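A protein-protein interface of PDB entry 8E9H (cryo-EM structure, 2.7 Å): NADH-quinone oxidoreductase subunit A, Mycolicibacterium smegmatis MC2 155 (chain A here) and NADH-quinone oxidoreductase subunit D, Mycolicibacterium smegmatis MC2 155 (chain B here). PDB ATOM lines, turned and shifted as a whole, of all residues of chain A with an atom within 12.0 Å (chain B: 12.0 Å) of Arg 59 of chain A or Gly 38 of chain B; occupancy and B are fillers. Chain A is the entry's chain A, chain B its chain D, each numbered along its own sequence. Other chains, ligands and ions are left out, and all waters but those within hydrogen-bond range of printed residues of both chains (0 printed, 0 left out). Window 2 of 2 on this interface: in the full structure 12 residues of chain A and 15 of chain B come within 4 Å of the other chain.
Hydrophobic or aromatic side chains of chain A that line the printed part of chain B: Ile 60 and Pro 61.
Of the 14 printed residues of chain B, 7 touch a printed residue of chain A.
Among the printed residues, 13 pairs touch across the chains.
Among the printed residues, no Asp or Glu carboxylate lies within 4 Å of a Lys or Arg side-chain nitrogen of the other chain.
O of Arg 40 of chain B lies within hydrogen-bond range of N of Gly 57 of chain A (3.0 Å).
The backbone NH of Gln 58 of chain A is in hydrogen-bond range of the backbone carbonyl oxygen of Gly 38 of chain B (3.3 Å).
The backbone carbonyl oxygen (O) of Gly 38 of chain B is in hydrogen-bond range of the backbone NH (N) of Arg 59 of chain A, at 3.1 Å.
Among the printed residues, pairs that only touch across the chains: Ile 60 of chain A with Ile 41 of chain B, Pro 61 of chain A with Gly 64 of chain B, Arg 63 of chain A with Ile 66 of chain B, Arg 59 of chain A with Glu 39 of chain B, Pro 61 of chain A with Glu 39 of chain B, Thr 56 of chain A with Arg 40 of chain B, Gly 57 of chain A with Ile 41 of chain B, Leu 55 of chain A with Ala 37 of chain B, Gly 57 of chain A with Gly 38 of chain B and Thr 56 of chain A with Ala 37 of chain B.
The guanidinium group of Arg 40 of chain B lies within salt-bridge range of the side-chain carboxylate of Glu 61 of chain B (2.8 Å).
The backbone carbonyl oxygen (O) of Ile 41 of chain B lies within hydrogen-bond range of the backbone NH (N) of Ile 62 of chain B, at 2.9 Å.
Arg 59 of chain A touches just these residues of chain B: Gly 38 and Glu 39.
Of chain A, only Gly 57, Gln 58 and Arg 59 come within 4 Å of Gly 38 of chain B.
Of chain B, only Ala 37 (3.6 Å) comes within 4 Å of Leu 55 of chain A.
Of chain B, only Ala 37 (3.9 Å) and Arg 40 (3.4 Å) come within 4 Å of Thr 56 of chain A.
Gln 58 of chain A touches just one residue of chain B: Gly 38.
Of the printed residues of chain B, Ile 60 of chain A touches Ile 41 (3.2 Å).
Pro 61 of chain A touches two residues of chain B.
No residue of chain A comes within 4 Å of Gln 36 of chain B.
Of chain A, only Leu 55 and Thr 56 come within 4 Å of Ala 37 of chain B.
Of chain A, only Arg 59 (3.3 Å) and Pro 61 (3.4 Å) come within 4 Å of Glu 39 of chain B.
Printed residues of chain A within 4 Å of Ile 66 of chain B: Arg 63 (3.3 Å).
Of the printed residues of chain A, Ile 41 of chain B touches Gly 57 and Ile 60.
Ala 53 of chain A touches none of the printed residues of chain B.
The nearest residue of chain B that does not touch Arg 59 of chain A is Arg 40 of chain B (4.6 Å).
The nearest residue of chain A that does not touch Gly 38 of chain B is Leu 55 of chain A (4.02 Å).
The nearest printed residue of chain A that does not touch Arg 40 of chain B is Arg 59 of chain A (4.6 Å).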
ATOM      1  N   LEU A  48     -13.702  -9.744  -0.135  1.00  0.00           N
ATOM      2  CA  LEU A  48     -12.980  -8.601   0.396  1.00  0.00           C
ATOM      3  C   LEU A  48     -12.867  -7.537  -0.691  1.00  0.00           C
ATOM      4  O   LEU A  48     -12.632  -7.880  -1.857  1.00  0.00           O
ATOM      5  CB  LEU A  48     -11.596  -9.032   0.876  1.00  0.00           C
ATOM      6  CG  LEU A  48     -10.762  -8.019   1.654  1.00  0.00           C
ATOM      7  CD1 LEU A  48     -11.391  -7.709   2.995  1.00  0.00           C
ATOM      8  CD2 LEU A  48      -9.360  -8.558   1.847  1.00  0.00           C
ATOM      9  N   ALA A  52      -9.263  -2.637  -2.344  1.00  0.00           N
ATOM     10  CA  ALA A  52      -8.186  -2.806  -1.377  1.00  0.00           C
ATOM     11  C   ALA A  52      -7.517  -4.171  -1.488  1.00  0.00           C
ATOM     12  O   ALA A  52      -7.011  -4.696  -0.487  1.00  0.00           O
ATOM     13  CB  ALA A  52      -8.717  -2.588   0.040  1.00  0.00           C
ATOM     14  N   ALA A  53      -7.508  -4.763  -2.685  1.00  0.00           N
ATOM     15  CA  ALA A  53      -6.910  -6.082  -2.858  1.00  0.00           C
ATOM     16  C   ALA A  53      -5.400  -6.050  -2.660  1.00  0.00           C
ATOM     17  O   ALA A  53      -4.826  -7.010  -2.134  1.00  0.00           O
ATOM     18  CB  ALA A  53      -7.243  -6.634  -4.242  1.00  0.00           C
ATOM     19  N   GLY A  54      -4.746  -4.966  -3.067  1.00  0.00           N
ATOM     20  CA  GLY A  54      -3.299  -4.900  -3.019  1.00  0.00           C
ATOM     21  C   GLY A  54      -2.741  -4.581  -1.648  1.00  0.00           C
ATOM     22  O   GLY A  54      -1.843  -3.744  -1.520  1.00  0.00           O
ATOM     23  N   LEU A  55      -3.264  -5.239  -0.613  1.00  0.00           N
ATOM     24  CA  LEU A  55      -2.754  -5.057   0.740  1.00  0.00           C
ATOM     25  C   LEU A  55      -2.535  -6.401   1.424  1.00  0.00           C
ATOM     26  O   LEU A  55      -1.719  -6.508   2.346  1.00  0.00           O
ATOM     27  CB  LEU A  55      -3.717  -4.199   1.561  1.00  0.00           C
ATOM     28  N   THR A  56      -3.250  -7.431   0.979  1.00  0.00           N
ATOM     29  CA  THR A  56      -3.166  -8.759   1.563  1.00  0.00           C
ATOM     30  C   THR A  56      -3.114  -9.805   0.459  1.00  0.00           C
ATOM     31  O   THR A  56      -3.639  -9.601  -0.639  1.00  0.00           O
ATOM     32  CB  THR A  56      -4.363  -9.049   2.477  1.00  0.00           C
ATOM     33  OG1 THR A  56      -5.533  -9.272   1.681  1.00  0.00           O
ATOM     34  CG2 THR A  56      -4.609  -7.885   3.422  1.00  0.00           C
ATOM     35  N   GLY A  57      -2.470 -10.928   0.762  1.00  0.00           N
ATOM     36  CA  GLY A  57      -2.401 -12.012  -0.194  1.00  0.00           C
ATOM     37  C   GLY A  57      -1.664 -11.670  -1.462  1.00  0.00           C
ATOM     38  O   GLY A  57      -1.778 -12.399  -2.450  1.00  0.00           O
ATOM     39  N   GLN A  58      -0.910 -10.571  -1.473  1.00  0.00           N
ATOM     40  CA  GLN A  58      -0.108 -10.255  -2.646  1.00  0.00           C
ATOM     41  C   GLN A  58       0.914 -11.350  -2.907  1.00  0.00           C
ATOM     42  O   GLN A  58       1.084 -11.792  -4.048  1.00  0.00           O
ATOM     43  CB  GLN A  58       0.582  -8.905  -2.462  1.00  0.00           C
ATOM     44  N   ARG A  59       1.585 -11.815  -1.858  1.00  0.00           N
ATOM     45  CA  ARG A  59       2.587 -12.866  -1.949  1.00  0.00           C
ATOM     46  C   ARG A  59       2.174 -14.016  -1.045  1.00  0.00           C
ATOM     47  O   ARG A  59       1.764 -13.792   0.097  1.00  0.00           O
ATOM     48  CB  ARG A  59       3.965 -12.342  -1.545  1.00  0.00           C
ATOM     49  CG  ARG A  59       4.690 -11.625  -2.663  1.00  0.00           C
ATOM     50  CD  ARG A  59       5.855 -10.801  -2.153  1.00  0.00           C
ATOM     51  NE  ARG A  59       5.416  -9.668  -1.349  1.00  0.00           N
ATOM     52  CZ  ARG A  59       5.365  -9.652  -0.025  1.00  0.00           C
ATOM     53  NH1 ARG A  59       5.723 -10.702   0.698  1.00  0.00           N
ATOM     54  NH2 ARG A  59       4.941  -8.553   0.593  1.00  0.00           N
ATOM     55  N   ILE A  60       2.283 -15.238  -1.553  1.00  0.00           N
ATOM     56  CA  ILE A  60       1.873 -16.420  -0.799  1.00  0.00           C
ATOM     57  C   ILE A  60       3.108 -17.229  -0.427  1.00  0.00           C
ATOM     58  O   ILE A  60       3.642 -17.955  -1.276  1.00  0.00           O
ATOM     59  CB  ILE A  60       0.892 -17.281  -1.606  1.00  0.00           C
ATOM     60  CG1 ILE A  60      -0.278 -16.432  -2.093  1.00  0.00           C
ATOM     61  CG2 ILE A  60       0.385 -18.433  -0.764  1.00  0.00           C
ATOM     62  CD1 ILE A  60      -0.916 -15.587  -1.022  1.00  0.00           C
ATOM     63  N   PRO A  61       3.592 -17.156   0.809  1.00  0.00           N
ATOM     64  CA  PRO A  61       4.759 -17.960   1.173  1.00  0.00           C
ATOM     65  C   PRO A  61       4.438 -19.442   1.104  1.00  0.00           C
ATOM     66  O   PRO A  61       3.313 -19.865   1.370  1.00  0.00           O
ATOM     67  CB  PRO A  61       5.070 -17.513   2.605  1.00  0.00           C
ATOM     68  CG  PRO A  61       3.800 -16.977   3.117  1.00  0.00           C
ATOM     69  CD  PRO A  61       3.094 -16.371   1.949  1.00  0.00           C
ATOM     70  N   ILE A  62       5.440 -20.227   0.733  1.00  0.00           N
ATOM     71  CA  ILE A  62       5.356 -21.680   0.752  1.00  0.00           C
ATOM     72  C   ILE A  62       6.367 -22.185   1.767  1.00  0.00           C
ATOM     73  O   ILE A  62       7.534 -21.780   1.750  1.00  0.00           O
ATOM     74  CB  ILE A  62       5.604 -22.280  -0.645  1.00  0.00           C
ATOM     75  CG1 ILE A  62       7.074 -22.147  -1.045  1.00  0.00           C
ATOM     76  CG2 ILE A  62       4.715 -21.599  -1.665  1.00  0.00           C
ATOM     77  CD1 ILE A  62       7.369 -22.640  -2.436  1.00  0.00           C
ATOM     78  N   ARG A  63       5.912 -23.045   2.670  1.00  0.00           N
ATOM     79  CA  ARG A  63       6.754 -23.527   3.751  1.00  0.00           C
ATOM     80  C   ARG A  63       7.672 -24.660   3.326  1.00  0.00           C
ATOM     81  O   ARG A  63       8.510 -25.091   4.123  1.00  0.00           O
ATOM     82  CB  ARG A  63       5.883 -23.980   4.925  1.00  0.00           C
ATOM     83  CG  ARG A  63       4.901 -22.917   5.364  1.00  0.00           C
ATOM     84  CD  ARG A  63       4.028 -23.378   6.507  1.00  0.00           C
ATOM     85  NE  ARG A  63       4.808 -23.906   7.620  1.00  0.00           N
ATOM     86  CZ  ARG A  63       4.855 -25.183   7.980  1.00  0.00           C
ATOM     87  NH1 ARG A  63       4.171 -26.114   7.335  1.00  0.00           N
ATOM     88  NH2 ARG A  63       5.605 -25.534   9.021  1.00  0.00           N
ATOM     89  N   TYR A  65       9.637 -24.353   0.470  1.00  0.00           N
ATOM     90  CA  TYR A  65      10.447 -23.780  -0.595  1.00  0.00           C
ATOM     91  C   TYR A  65      11.782 -24.498  -0.707  1.00  0.00           C
ATOM     92  O   TYR A  65      12.327 -24.655  -1.803  1.00  0.00           O
ATOM     93  CB  TYR A  65      10.664 -22.289  -0.348  1.00  0.00           C
ATOM     94  CG  TYR A  65      11.319 -21.977   0.970  1.00  0.00           C
ATOM     95  CD1 TYR A  65      10.562 -21.706   2.096  1.00  0.00           C
ATOM     96  CD2 TYR A  65      12.696 -21.953   1.091  1.00  0.00           C
ATOM     97  CE1 TYR A  65      11.155 -21.420   3.300  1.00  0.00           C
ATOM     98  CE2 TYR A  65      13.298 -21.668   2.291  1.00  0.00           C
ATOM     99  CZ  TYR A  65      12.523 -21.402   3.391  1.00  0.00           C
ATOM    100  OH  TYR A  65      13.122 -21.116   4.593  1.00  0.00           O
ATOM    101  N   GLN B  36       4.810 -10.168   7.125  1.00  0.00           N
ATOM    102  CA  GLN B  36       4.049  -8.932   7.250  1.00  0.00           C
ATOM    103  C   GLN B  36       2.684  -9.070   6.590  1.00  0.00           C
ATOM    104  O   GLN B  36       2.240 -10.174   6.286  1.00  0.00           O
ATOM    105  CB  GLN B  36       4.817  -7.764   6.630  1.00  0.00           C
ATOM    106  N   ALA B  37       2.023  -7.933   6.365  1.00  0.00           N
ATOM    107  CA  ALA B  37       0.682  -7.959   5.789  1.00  0.00           C
ATOM    108  C   ALA B  37       0.689  -8.552   4.388  1.00  0.00           C
ATOM    109  O   ALA B  37      -0.217  -9.308   4.020  1.00  0.00           O
ATOM    110  CB  ALA B  37       0.099  -6.547   5.764  1.00  0.00           C
ATOM    111  N   GLY B  38       1.703  -8.222   3.590  1.00  0.00           N
ATOM    112  CA  GLY B  38       1.744  -8.690   2.218  1.00  0.00           C
ATOM    113  C   GLY B  38       1.735 -10.197   2.080  1.00  0.00           C
ATOM    114  O   GLY B  38       1.288 -10.713   1.051  1.00  0.00           O
ATOM    115  N   GLU B  39       2.211 -10.917   3.092  1.00  0.00           N
ATOM    116  CA  GLU B  39       2.319 -12.367   3.032  1.00  0.00           C
ATOM    117  C   GLU B  39       1.168 -13.079   3.731  1.00  0.00           C
ATOM    118  O   GLU B  39       1.200 -14.305   3.852  1.00  0.00           O
ATOM    119  CB  GLU B  39       3.647 -12.816   3.641  1.00  0.00           C
ATOM    120  N   ARG B  40       0.156 -12.347   4.186  1.00  0.00           N
ATOM    121  CA  ARG B  40      -0.956 -12.917   4.934  1.00  0.00           C
ATOM    122  C   ARG B  40      -2.238 -12.774   4.131  1.00  0.00           C
ATOM    123  O   ARG B  40      -2.575 -11.670   3.690  1.00  0.00           O
ATOM    124  CB  ARG B  40      -1.116 -12.227   6.286  1.00  0.00           C
ATOM    125  CG  ARG B  40       0.064 -12.380   7.213  1.00  0.00           C
ATOM    126  CD  ARG B  40       0.054 -13.729   7.891  1.00  0.00           C
ATOM    127  NE  ARG B  40       1.198 -13.897   8.776  1.00  0.00           N
ATOM    128  CZ  ARG B  40       1.360 -13.245   9.919  1.00  0.00           C
ATOM    129  NH1 ARG B  40       0.462 -12.377  10.354  1.00  0.00           N
ATOM    130  NH2 ARG B  40       2.449 -13.472  10.645  1.00  0.00           N
ATOM    131  N   ILE B  41      -2.948 -13.882   3.944  1.00  0.00           N
ATOM    132  CA  ILE B  41      -4.320 -13.813   3.466  1.00  0.00           C
ATOM    133  C   ILE B  41      -5.261 -13.876   4.661  1.00  0.00           C
ATOM    134  O   ILE B  41      -4.919 -14.387   5.725  1.00  0.00           O
ATOM    135  CB  ILE B  41      -4.626 -14.941   2.468  1.00  0.00           C
ATOM    136  CG1 ILE B  41      -3.778 -14.803   1.209  1.00  0.00           C
ATOM    137  CG2 ILE B  41      -6.098 -14.924   2.093  1.00  0.00           C
ATOM    138  CD1 ILE B  41      -3.777 -16.049   0.353  1.00  0.00           C
ATOM    139  N   VAL B  42      -6.459 -13.335   4.488  1.00  0.00           N
ATOM    140  CA  VAL B  42      -7.544 -13.534   5.437  1.00  0.00           C
ATOM    141  C   VAL B  42      -8.723 -14.103   4.665  1.00  0.00           C
ATOM    142  O   VAL B  42      -9.208 -13.481   3.716  1.00  0.00           O
ATOM    143  CB  VAL B  42      -7.924 -12.234   6.166  1.00  0.00           C
ATOM    144  CG1 VAL B  42      -8.332 -11.164   5.182  1.00  0.00           C
ATOM    145  CG2 VAL B  42      -9.035 -12.497   7.156  1.00  0.00           C
ATOM    146  N   GLU B  61      -6.854 -15.910   9.409  1.00  0.00           N
ATOM    147  CA  GLU B  61      -5.703 -15.249   8.823  1.00  0.00           C
ATOM    148  C   GLU B  61      -4.578 -16.263   8.701  1.00  0.00           C
ATOM    149  O   GLU B  61      -4.117 -16.809   9.709  1.00  0.00           O
ATOM    150  CB  GLU B  61      -5.265 -14.071   9.686  1.00  0.00           C
ATOM    151  CG  GLU B  61      -4.108 -13.282   9.116  1.00  0.00           C
ATOM    152  CD  GLU B  61      -3.589 -12.245  10.085  1.00  0.00           C
ATOM    153  OE1 GLU B  61      -4.412 -11.605  10.770  1.00  0.00           O
ATOM    154  OE2 GLU B  61      -2.356 -12.074  10.167  1.00  0.00           O
ATOM    155  N   ILE B  62      -4.141 -16.509   7.469  1.00  0.00           N
ATOM    156  CA  ILE B  62      -3.211 -17.582   7.148  1.00  0.00           C
ATOM    157  C   ILE B  62      -1.988 -16.995   6.460  1.00  0.00           C
ATOM    158  O   ILE B  62      -2.114 -16.202   5.519  1.00  0.00           O
ATOM    159  CB  ILE B  62      -3.876 -18.648   6.258  1.00  0.00           C
ATOM    160  CG1 ILE B  62      -4.134 -18.095   4.857  1.00  0.00           C
ATOM    161  CG2 ILE B  62      -5.176 -19.108   6.874  1.00  0.00           C
ATOM    162  CD1 ILE B  62      -4.956 -19.012   3.993  1.00  0.00           C
ATOM    163  N   GLU B  63      -0.809 -17.382   6.937  1.00  0.00           N
ATOM    164  CA  GLU B  63       0.454 -17.106   6.261  1.00  0.00           C
ATOM    165  C   GLU B  63       0.815 -18.375   5.499  1.00  0.00           C
ATOM    166  O   GLU B  63       1.203 -19.380   6.096  1.00  0.00           O
ATOM    167  CB  GLU B  63       1.542 -16.716   7.254  1.00  0.00           C
ATOM    168  N   GLY B  64       0.680 -18.331   4.179  1.00  0.00           N
ATOM    169  CA  GLY B  64       0.806 -19.540   3.396  1.00  0.00           C
ATOM    170  C   GLY B  64      -0.411 -20.412   3.603  1.00  0.00           C
ATOM    171  O   GLY B  64      -1.497 -20.094   3.112  1.00  0.00           O
ATOM    172  N   GLU B  65      -0.246 -21.517   4.327  1.00  0.00           N
ATOM    173  CA  GLU B  65      -1.391 -22.316   4.740  1.00  0.00           C
ATOM    174  C   GLU B  65      -1.400 -22.568   6.242  1.00  0.00           C
ATOM    175  O   GLU B  65      -2.146 -23.441   6.699  1.00  0.00           O
ATOM    176  CB  GLU B  65      -1.424 -23.645   3.982  1.00  0.00           C
ATOM    177  CG  GLU B  65      -2.800 -24.292   3.953  1.00  0.00           C
ATOM    178  CD  GLU B  65      -3.020 -25.171   2.737  1.00  0.00           C
ATOM    179  OE1 GLU B  65      -2.396 -24.911   1.688  1.00  0.00           O
ATOM    180  OE2 GLU B  65      -3.818 -26.126   2.829  1.00  0.00           O
ATOM    181  N   ILE B  66      -0.604 -21.839   7.014  1.00  0.00           N
ATOM    182  CA  ILE B  66      -0.622 -21.946   8.467  1.00  0.00           C
ATOM    183  C   ILE B  66      -1.608 -20.928   9.018  1.00  0.00           C
ATOM    184  O   ILE B  66      -1.561 -19.747   8.658  1.00  0.00           O
ATOM    185  CB  ILE B  66       0.782 -21.719   9.043  1.00  0.00           C
ATOM    186  CG1 ILE B  66       1.681 -22.919   8.756  1.00  0.00           C
ATOM    187  CG2 ILE B  66       0.708 -21.465  10.532  1.00  0.00           C
ATOM    188  CD1 ILE B  66       1.400 -24.126   9.614  1.00  0.00           C
ATOM    189  N   THR B  68      -2.550 -18.334  11.089  1.00  0.00           N
ATOM    190  CA  THR B  68      -1.917 -17.394  12.005  1.00  0.00           C
ATOM    191  C   THR B  68      -2.903 -16.866  13.036  1.00  0.00           C
ATOM    192  O   THR B  68      -2.525 -16.609  14.183  1.00  0.00           O
ATOM    193  CB  THR B  68      -1.305 -16.233  11.228  1.00  0.00           C
ATOM    194  OG1 THR B  68      -0.367 -16.737  10.271  1.00  0.00           O
ATOM    195  CG2 THR B  68      -0.602 -15.279  12.174  1.00  0.00           C
